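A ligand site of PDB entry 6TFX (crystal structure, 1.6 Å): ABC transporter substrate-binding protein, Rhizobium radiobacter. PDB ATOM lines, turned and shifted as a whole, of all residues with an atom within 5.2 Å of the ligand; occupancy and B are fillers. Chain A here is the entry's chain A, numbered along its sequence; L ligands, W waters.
The side-chain hydroxyl (OH) of Tyr 384 sits at hydrogen-bond distance from the guanidinium group (NH2) of Arg 375. The side-chain amide oxygen of Asn 251 is in hydrogen-bond range of the side-chain amide nitrogen of Asn 460 (2.8 Å). The backbone carbonyl oxygen (O) of Glu 249 lies within hydrogen-bond range of the backbone NH (N) of Asn 460. A ring nitrogen (NE2) of His 371 lies within hydrogen-bond range of a ring nitrogen (NE2) of His 367, 3.2 Å away. ND1 of His 371 is in hydrogen-bond range of NH1 of Arg 375 (2.8 Å). The guanidinium group of Arg 284 sits at hydrogen-bond distance from the backbone carbonyl oxygen of Gly 341 (3.0 Å). The guanidinium group (NE) of Arg 29 is in hydrogen-bond range of the backbone carbonyl oxygen (O) of Thr 24 (2.8 Å).
OH of Tyr 384 sits at hydrogen-bond distance from O8 of the ligand (2.6 Å). The side-chain amide nitrogen (ND2) of Asn 251 lies within hydrogen-bond range of an oxygen (O3) of the ligand. The side-chain carboxylate of Glu 249 is in salt-bridge range of a nitrogen (N1) of the ligand (2.7 Å). An oxygen (O9) of the ligand sits at hydrogen-bond distance from a ring nitrogen (NE2) of His 367. A ring nitrogen (NE2) of His 371 sits at hydrogen-bond distance from an oxygen (O6) of the ligand, at 2.8 Å. An oxygen (O8) of the ligand is in salt-bridge range of the guanidinium group (NH2) of Arg 388, 2.8 Å away. The guanidinium group (NH1) of Arg 284 lies within hydrogen-bond range of an oxygen (O1) of the ligand, 2.8 Å away. The backbone carbonyl oxygen (O) of Gly 385 sits close to a nitrogen (N1) of the ligand (3.5 Å). OE1 of Gln 226 sits at hydrogen-bond distance from O1 of the ligand, at 2.9 Å. An oxygen (O9) of the ligand sits at hydrogen-bond distance from the backbone NH (N) of Thr 26 (3.0 Å). The side-chain hydroxyl of Thr 26 sits at hydrogen-bond distance from a nitrogen (N1) of the ligand. O of Gly 341 sits at hydrogen-bond distance from O1 of the ligand (3.0 Å). O7 of the ligand is in salt-bridge range of NH2 of Arg 29 (3.0 Å). The side-chain amide oxygen (OD1) of Asn 460 is in hydrogen-bond range of an oxygen (O3) of the ligand, 3.1 Å away.
The backbone carbonyl oxygen (O) of Thr 24 lies close to an oxygen (O7) of the ligand. CA of Thr 25 touches O9 of the ligand, at 3.4 Å. Leu 339 touches the ligand (CD2 to C6, 3.9 Å). Leu 342 touches the ligand. Hydrophobic or aromatic side chains within 4 Å of the ligand: Leu 339, Leu 342, His 367, His 371 and Tyr 384. Of the 23 residues printed, 17 come within 4 Å of the ligand. The nearest printed residue that does not touch the ligand is Ala 386 (4.03 Å).
Water W3 bridges an oxygen (O7) of the ligand and the guanidinium group of Arg 29. Water W2 lies within hydrogen-bond range of an oxygen (O6) of the ligand (2.9 Å) and the backbone NH of Gly 385 (3.0 Å). Water W1 bridges the side-chain amide nitrogen of Gln 226 (2.9 Å) and an oxygen (O4) of the ligand (3.0 Å). Water W5 lies within hydrogen-bond range of the side-chain hydroxyl (OG1) of Thr 26, the side-chain carboxylate (OE1) of Glu 249 and an oxygen (O4) of the ligand.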
ATOM      1  N   THR A  24      -4.525  -6.335 -17.865  1.00  0.00           N
ATOM      2  CA  THR A  24      -3.621  -5.181 -17.945  1.00  0.00           C
ATOM      3  C   THR A  24      -2.738  -4.999 -16.722  1.00  0.00           C
ATOM      4  O   THR A  24      -1.562  -4.656 -16.871  1.00  0.00           O
ATOM      5  CB  THR A  24      -4.472  -3.925 -18.193  1.00  0.00           C
ATOM      6  OG1 THR A  24      -5.219  -4.107 -19.401  1.00  0.00           O
ATOM      7  CG2 THR A  24      -3.644  -2.645 -18.269  1.00  0.00           C
ATOM      8  N   THR A  25      -3.288  -5.219 -15.502  1.00  0.00           N
ATOM      9  CA  THR A  25      -2.439  -5.052 -14.315  1.00  0.00           C
ATOM     10  C   THR A  25      -1.345  -6.120 -14.335  1.00  0.00           C
ATOM     11  O   THR A  25      -1.548  -7.204 -14.917  1.00  0.00           O
ATOM     12  CB  THR A  25      -3.271  -5.159 -13.042  1.00  0.00           C
ATOM     13  OG1 THR A  25      -3.728  -6.500 -12.921  1.00  0.00           O
ATOM     14  CG2 THR A  25      -4.470  -4.171 -13.006  1.00  0.00           C
ATOM     15  N   THR A  26      -0.218  -5.850 -13.667  1.00  0.00           N
ATOM     16  CA  THR A  26       0.846  -6.875 -13.636  1.00  0.00           C
ATOM     17  C   THR A  26       0.289  -8.199 -13.089  1.00  0.00           C
ATOM     18  O   THR A  26       0.599  -9.275 -13.634  1.00  0.00           O
ATOM     19  CB  THR A  26       2.008  -6.397 -12.768  1.00  0.00           C
ATOM     20  OG1 THR A  26       2.642  -5.325 -13.440  1.00  0.00           O
ATOM     21  CG2 THR A  26       3.044  -7.491 -12.535  1.00  0.00           C
ATOM     22  N   ARG A  29      -1.834  -9.964 -15.705  1.00  0.00           N
ATOM     23  CA  ARG A  29      -0.971 -10.425 -16.812  1.00  0.00           C
ATOM     24  C   ARG A  29      -0.103 -11.633 -16.368  1.00  0.00           C
ATOM     25  O   ARG A  29       0.216 -12.498 -17.195  1.00  0.00           O
ATOM     26  CB  ARG A  29      -0.033  -9.311 -17.291  1.00  0.00           C
ATOM     27  CG  ARG A  29      -0.765  -8.161 -17.975  1.00  0.00           C
ATOM     28  CD  ARG A  29       0.283  -7.169 -18.417  1.00  0.00           C
ATOM     29  NE  ARG A  29      -0.240  -5.944 -19.015  1.00  0.00           N
ATOM     30  CZ  ARG A  29      -0.462  -5.752 -20.312  1.00  0.00           C
ATOM     31  NH1 ARG A  29      -0.332  -6.753 -21.184  1.00  0.00           N
ATOM     32  NH2 ARG A  29      -0.858  -4.563 -20.758  1.00  0.00           N
ATOM     33  N   GLN A 226      10.633  -1.267  -5.159  1.00  0.00           N
ATOM     34  CA  GLN A 226      11.755  -0.586  -5.837  1.00  0.00           C
ATOM     35  C   GLN A 226      12.807  -0.021  -4.900  1.00  0.00           C
ATOM     36  O   GLN A 226      13.806   0.551  -5.347  1.00  0.00           O
ATOM     37  CB  GLN A 226      11.199   0.541  -6.726  1.00  0.00           C
ATOM     38  CG  GLN A 226      10.280   0.061  -7.852  1.00  0.00           C
ATOM     39  CD  GLN A 226       8.903  -0.375  -7.378  1.00  0.00           C
ATOM     40  OE1 GLN A 226       8.284   0.285  -6.518  1.00  0.00           O
ATOM     41  NE2 GLN A 226       8.416  -1.495  -7.887  1.00  0.00           N
ATOM     42  N   GLU A 249       9.937  -0.962 -16.315  1.00  0.00           N
ATOM     43  CA  GLU A 249       8.690  -0.250 -16.605  1.00  0.00           C
ATOM     44  C   GLU A 249       8.920   1.244 -16.358  1.00  0.00           C
ATOM     45  O   GLU A 249       9.418   1.612 -15.292  1.00  0.00           O
ATOM     46  CB  GLU A 249       7.571  -0.753 -15.667  1.00  0.00           C
ATOM     47  CG  GLU A 249       7.242  -2.207 -15.908  1.00  0.00           C
ATOM     48  CD  GLU A 249       6.114  -2.652 -14.990  1.00  0.00           C
ATOM     49  OE1 GLU A 249       6.401  -2.953 -13.812  1.00  0.00           O
ATOM     50  OE2 GLU A 249       4.957  -2.676 -15.447  1.00  0.00           O
ATOM     51  N   ASN A 251       7.846   5.001 -15.536  1.00  0.00           N
ATOM     52  CA  ASN A 251       6.806   5.757 -14.859  1.00  0.00           C
ATOM     53  C   ASN A 251       6.815   7.170 -15.400  1.00  0.00           C
ATOM     54  O   ASN A 251       7.897   7.774 -15.494  1.00  0.00           O
ATOM     55  CB  ASN A 251       7.113   5.813 -13.360  1.00  0.00           C
ATOM     56  CG  ASN A 251       7.344   4.441 -12.788  1.00  0.00           C
ATOM     57  OD1 ASN A 251       8.473   4.070 -12.387  1.00  0.00           O
ATOM     58  ND2 ASN A 251       6.298   3.634 -12.802  1.00  0.00           N
ATOM     59  N   ARG A 284      15.939   5.398  -4.501  1.00  0.00           N
ATOM     60  CA  ARG A 284      15.436   4.019  -4.626  1.00  0.00           C
ATOM     61  C   ARG A 284      16.531   3.003  -4.888  1.00  0.00           C
ATOM     62  O   ARG A 284      16.408   1.871  -4.427  1.00  0.00           O
ATOM     63  CB  ARG A 284      14.350   3.930  -5.710  1.00  0.00           C
ATOM     64  CG  ARG A 284      13.062   4.592  -5.263  1.00  0.00           C
ATOM     65  CD  ARG A 284      11.971   4.468  -6.328  1.00  0.00           C
ATOM     66  NE  ARG A 284      10.671   4.423  -5.688  1.00  0.00           N
ATOM     67  CZ  ARG A 284       9.539   4.087  -6.310  1.00  0.00           C
ATOM     68  NH1 ARG A 284       9.532   3.813  -7.607  1.00  0.00           N
ATOM     69  NH2 ARG A 284       8.390   4.020  -5.629  1.00  0.00           N
ATOM     70  N   LEU A 339      -1.362   0.539  -5.445  1.00  0.00           N
ATOM     71  CA  LEU A 339      -0.275  -0.439  -5.680  1.00  0.00           C
ATOM     72  C   LEU A 339       0.906   0.176  -4.912  1.00  0.00           C
ATOM     73  O   LEU A 339       1.191   1.358  -5.117  1.00  0.00           O
ATOM     74  CB  LEU A 339       0.044  -0.545  -7.175  1.00  0.00           C
ATOM     75  CG  LEU A 339       1.192  -1.504  -7.548  1.00  0.00           C
ATOM     76  CD1 LEU A 339       0.816  -2.951  -7.265  1.00  0.00           C
ATOM     77  CD2 LEU A 339       1.557  -1.339  -9.019  1.00  0.00           C
ATOM     78  N   GLY A 341       4.168   0.389  -4.864  1.00  0.00           N
ATOM     79  CA  GLY A 341       5.249   1.041  -5.604  1.00  0.00           C
ATOM     80  C   GLY A 341       4.805   2.344  -6.250  1.00  0.00           C
ATOM     81  O   GLY A 341       5.547   3.331  -6.213  1.00  0.00           O
ATOM     82  N   LEU A 342       3.565   2.371  -6.804  1.00  0.00           N
ATOM     83  CA  LEU A 342       3.020   3.599  -7.402  1.00  0.00           C
ATOM     84  C   LEU A 342       2.614   4.587  -6.308  1.00  0.00           C
ATOM     85  O   LEU A 342       2.746   5.803  -6.468  1.00  0.00           O
ATOM     86  CB  LEU A 342       1.783   3.299  -8.279  1.00  0.00           C
ATOM     87  CG  LEU A 342       2.100   2.751  -9.658  1.00  0.00           C
ATOM     88  CD1 LEU A 342       0.820   2.296 -10.347  1.00  0.00           C
ATOM     89  CD2 LEU A 342       2.862   3.773 -10.517  1.00  0.00           C
ATOM     90  N   LEU A 345       5.827   6.105  -5.044  1.00  0.00           N
ATOM     91  CA  LEU A 345       6.349   7.027  -6.059  1.00  0.00           C
ATOM     92  C   LEU A 345       5.529   8.344  -6.062  1.00  0.00           C
ATOM     93  O   LEU A 345       6.105   9.432  -6.092  1.00  0.00           O
ATOM     94  CB  LEU A 345       6.319   6.392  -7.456  1.00  0.00           C
ATOM     95  CG  LEU A 345       6.929   7.235  -8.593  1.00  0.00           C
ATOM     96  CD1 LEU A 345       8.379   7.685  -8.292  1.00  0.00           C
ATOM     97  CD2 LEU A 345       6.939   6.458  -9.861  1.00  0.00           C
ATOM     98  N   HIS A 367      -5.785  -0.455  -6.937  1.00  0.00           N
ATOM     99  CA  HIS A 367      -5.123  -0.463  -8.252  1.00  0.00           C
ATOM    100  C   HIS A 367      -6.055  -0.773  -9.447  1.00  0.00           C
ATOM    101  O   HIS A 367      -6.052  -0.017 -10.435  1.00  0.00           O
ATOM    102  CB  HIS A 367      -3.933  -1.428  -8.227  1.00  0.00           C
ATOM    103  CG  HIS A 367      -3.033  -1.382  -9.427  1.00  0.00           C
ATOM    104  ND1 HIS A 367      -2.384  -0.214  -9.795  1.00  0.00           N
ATOM    105  CD2 HIS A 367      -2.655  -2.378 -10.269  1.00  0.00           C
ATOM    106  CE1 HIS A 367      -1.636  -0.525 -10.847  1.00  0.00           C
ATOM    107  NE2 HIS A 367      -1.798  -1.810 -11.197  1.00  0.00           N
ATOM    108  N   TRP A 370      -8.555   1.950  -9.923  1.00  0.00           N
ATOM    109  CA  TRP A 370      -7.850   3.136 -10.412  1.00  0.00           C
ATOM    110  C   TRP A 370      -7.660   3.016 -11.945  1.00  0.00           C
ATOM    111  O   TRP A 370      -7.931   3.972 -12.657  1.00  0.00           O
ATOM    112  CB  TRP A 370      -6.504   3.252  -9.699  1.00  0.00           C
ATOM    113  CG  TRP A 370      -5.559   4.254 -10.296  1.00  0.00           C
ATOM    114  CD1 TRP A 370      -5.578   5.607 -10.116  1.00  0.00           C
ATOM    115  CD2 TRP A 370      -4.451   3.960 -11.141  1.00  0.00           C
ATOM    116  NE1 TRP A 370      -4.516   6.186 -10.786  1.00  0.00           N
ATOM    117  CE2 TRP A 370      -3.794   5.190 -11.416  1.00  0.00           C
ATOM    118  CE3 TRP A 370      -3.918   2.773 -11.664  1.00  0.00           C
ATOM    119  CZ2 TRP A 370      -2.639   5.269 -12.220  1.00  0.00           C
ATOM    120  CZ3 TRP A 370      -2.756   2.835 -12.414  1.00  0.00           C
ATOM    121  CH2 TRP A 370      -2.142   4.078 -12.718  1.00  0.00           C
ATOM    122  N   HIS A 371      -7.259   1.816 -12.441  1.00  0.00           N
ATOM    123  CA  HIS A 371      -7.108   1.570 -13.878  1.00  0.00           C
ATOM    124  C   HIS A 371      -8.417   1.882 -14.620  1.00  0.00           C
ATOM    125  O   HIS A 371      -8.386   2.400 -15.721  1.00  0.00           O
ATOM    126  CB  HIS A 371      -6.731   0.098 -14.144  1.00  0.00           C
ATOM    127  CG  HIS A 371      -5.262  -0.114 -14.226  1.00  0.00           C
ATOM    128  ND1 HIS A 371      -4.560   0.153 -15.386  1.00  0.00           N
ATOM    129  CD2 HIS A 371      -4.392  -0.539 -13.276  1.00  0.00           C
ATOM    130  CE1 HIS A 371      -3.285  -0.128 -15.120  1.00  0.00           C
ATOM    131  NE2 HIS A 371      -3.134  -0.541 -13.867  1.00  0.00           N
ATOM    132  N   ARG A 375      -9.213   5.552 -17.113  1.00  0.00           N
ATOM    133  CA  ARG A 375      -9.714   5.295 -18.482  1.00  0.00           C
ATOM    134  C   ARG A 375     -11.093   5.938 -18.721  1.00  0.00           C
ATOM    135  O   ARG A 375     -11.655   5.787 -19.807  1.00  0.00           O
ATOM    136  CB  ARG A 375      -9.699   3.782 -18.764  1.00  0.00           C
ATOM    137  CG  ARG A 375      -8.268   3.296 -19.001  1.00  0.00           C
ATOM    138  CD  ARG A 375      -8.223   1.797 -19.104  1.00  0.00           C
ATOM    139  NE  ARG A 375      -6.907   1.273 -19.480  1.00  0.00           N
ATOM    140  CZ  ARG A 375      -5.892   1.144 -18.645  1.00  0.00           C
ATOM    141  NH1 ARG A 375      -5.980   1.591 -17.392  1.00  0.00           N
ATOM    142  NH2 ARG A 375      -4.746   0.596 -19.066  1.00  0.00           N
ATOM    143  N   TYR A 384       1.508   6.702 -14.373  1.00  0.00           N
ATOM    144  CA  TYR A 384       1.324   5.357 -14.923  1.00  0.00           C
ATOM    145  C   TYR A 384       2.734   4.792 -15.162  1.00  0.00           C
ATOM    146  O   TYR A 384       3.631   5.508 -15.622  1.00  0.00           O
ATOM    147  CB  TYR A 384       0.614   5.479 -16.282  1.00  0.00           C
ATOM    148  CG  TYR A 384      -0.087   4.215 -16.729  1.00  0.00           C
ATOM    149  CD1 TYR A 384      -1.394   3.927 -16.304  1.00  0.00           C
ATOM    150  CD2 TYR A 384       0.542   3.305 -17.581  1.00  0.00           C
ATOM    151  CE1 TYR A 384      -2.044   2.770 -16.731  1.00  0.00           C
ATOM    152  CE2 TYR A 384      -0.096   2.132 -17.995  1.00  0.00           C
ATOM    153  CZ  TYR A 384      -1.383   1.858 -17.538  1.00  0.00           C
ATOM    154  OH  TYR A 384      -2.066   0.755 -17.981  1.00  0.00           O
ATOM    155  N   GLY A 385       2.899   3.499 -14.902  1.00  0.00           N
ATOM    156  CA  GLY A 385       4.200   2.861 -15.113  1.00  0.00           C
ATOM    157  C   GLY A 385       4.019   1.607 -15.936  1.00  0.00           C
ATOM    158  O   GLY A 385       3.251   0.715 -15.555  1.00  0.00           O
ATOM    159  N   ALA A 386       4.707   1.518 -17.078  1.00  0.00           N
ATOM    160  CA  ALA A 386       4.534   0.325 -17.934  1.00  0.00           C
ATOM    161  C   ALA A 386       5.670   0.206 -18.916  1.00  0.00           C
ATOM    162  O   ALA A 386       6.405   1.178 -19.160  1.00  0.00           O
ATOM    163  CB  ALA A 386       3.246   0.463 -18.737  1.00  0.00           C
ATOM    164  N   ALA A 387       5.783  -0.986 -19.510  1.00  0.00           N
ATOM    165  CA  ALA A 387       6.686  -1.247 -20.621  1.00  0.00           C
ATOM    166  C   ALA A 387       5.848  -1.893 -21.735  1.00  0.00           C
ATOM    167  O   ALA A 387       4.793  -2.477 -21.450  1.00  0.00           O
ATOM    168  CB  ALA A 387       7.836  -2.178 -20.230  1.00  0.00           C
ATOM    169  N   ARG A 388       6.337  -1.820 -22.988  1.00  0.00           N
ATOM    170  CA  ARG A 388       5.643  -2.469 -24.092  1.00  0.00           C
ATOM    171  C   ARG A 388       6.719  -3.187 -24.924  1.00  0.00           C
ATOM    172  O   ARG A 388       7.913  -3.146 -24.551  1.00  0.00           O
ATOM    173  CB  ARG A 388       4.878  -1.416 -24.939  1.00  0.00           C
ATOM    174  CG  ARG A 388       3.646  -0.817 -24.218  1.00  0.00           C
ATOM    175  CD  ARG A 388       2.583  -1.907 -23.977  1.00  0.00           C
ATOM    176  NE  ARG A 388       1.332  -1.403 -23.392  1.00  0.00           N
ATOM    177  CZ  ARG A 388       1.012  -1.528 -22.109  1.00  0.00           C
ATOM    178  NH1 ARG A 388       1.890  -1.995 -21.234  1.00  0.00           N
ATOM    179  NH2 ARG A 388      -0.197  -1.143 -21.687  1.00  0.00           N
ATOM    180  N   VAL A 413      -3.964   4.207 -23.909  1.00  0.00           N
ATOM    181  CA  VAL A 413      -3.473   4.783 -22.654  1.00  0.00           C
ATOM    182  C   VAL A 413      -2.933   6.211 -22.869  1.00  0.00           C
ATOM    183  O   VAL A 413      -2.023   6.633 -22.144  1.00  0.00           O
ATOM    184  CB  VAL A 413      -2.448   3.855 -21.955  1.00  0.00           C
ATOM    185  CG1 VAL A 413      -3.152   2.675 -21.265  1.00  0.00           C
ATOM    186  CG2 VAL A 413      -1.409   3.336 -22.933  1.00  0.00           C
ATOM    187  N   ASN A 460      11.790   1.096 -13.672  1.00  0.00           N
ATOM    188  CA  ASN A 460      12.273   0.131 -12.672  1.00  0.00           C
ATOM    189  C   ASN A 460      12.139  -1.314 -13.182  1.00  0.00           C
ATOM    190  O   ASN A 460      11.098  -1.705 -13.736  1.00  0.00           O
ATOM    191  CB  ASN A 460      11.482   0.252 -11.351  1.00  0.00           C
ATOM    192  CG  ASN A 460      10.025   0.628 -11.532  1.00  0.00           C
ATOM    193  OD1 ASN A 460       9.181  -0.139 -12.051  1.00  0.00           O
ATOM    194  ND2 ASN A 460       9.725   1.839 -11.157  1.00  0.00           N
HETATM  195  O1  LIG L   1       7.317   2.279  -8.422  1.00  0.00           O
HETATM  196  C1  LIG L   1       6.662   2.216  -9.706  1.00  0.00           C
HETATM  197  C2  LIG L   1       5.526   1.153  -9.875  1.00  0.00           C
HETATM  198  O2  LIG L   1       5.517   0.186  -8.876  1.00  0.00           O
HETATM  199  C3  LIG L   1       5.371   0.727 -11.339  1.00  0.00           C
HETATM  200  O3  LIG L   1       6.340   0.998 -12.278  1.00  0.00           O
HETATM  201  C4  LIG L   1       5.050  -0.593 -12.004  1.00  0.00           C
HETATM  202  O4  LIG L   1       5.545  -1.667 -11.241  1.00  0.00           O
HETATM  203  C5  LIG L   1       3.631  -0.655 -12.491  1.00  0.00           C
HETATM  204  O5  LIG L   1       3.035   0.425 -12.745  1.00  0.00           O
HETATM  205  C6  LIG L   1       2.908  -2.027 -12.618  1.00  0.00           C
HETATM  206  N1  LIG L   1       2.663  -2.362 -14.002  1.00  0.00           N
HETATM  207  C7  LIG L   1       1.362  -2.479 -14.540  1.00  0.00           C
HETATM  208  C8  LIG L   1       0.208  -1.934 -13.730  1.00  0.00           C
HETATM  209  O6  LIG L   1      -0.383  -0.790 -13.698  1.00  0.00           O
HETATM  210  C9  LIG L   1       1.380  -2.087 -16.019  1.00  0.00           C
HETATM  211  C10 LIG L   1       0.098  -1.612 -16.688  1.00  0.00           C
HETATM  212  C11 LIG L   1       0.042  -1.914 -18.196  1.00  0.00           C
HETATM  213  O7  LIG L   1       0.632  -2.924 -18.696  1.00  0.00           O
HETATM  214  O8  LIG L   1      -0.617  -1.147 -18.929  1.00  0.00           O
HETATM  215  O9  LIG L   1      -0.141  -2.933 -13.083  1.00  0.00           O
HETATM  216  O   HOH W   1       7.919  -3.161 -10.231  1.00  0.00           O
HETATM  217  O   HOH W   2       0.486   1.967 -14.150  1.00  0.00           O
HETATM  218  O   HOH W   3       2.567  -4.929 -18.329  1.00  0.00           O
HETATM  219  O   HOH W   4       5.099  -2.546  -8.305  1.00  0.00           O
HETATM  220  O   HOH W   5       5.122  -4.888 -12.214  1.00  0.00           O
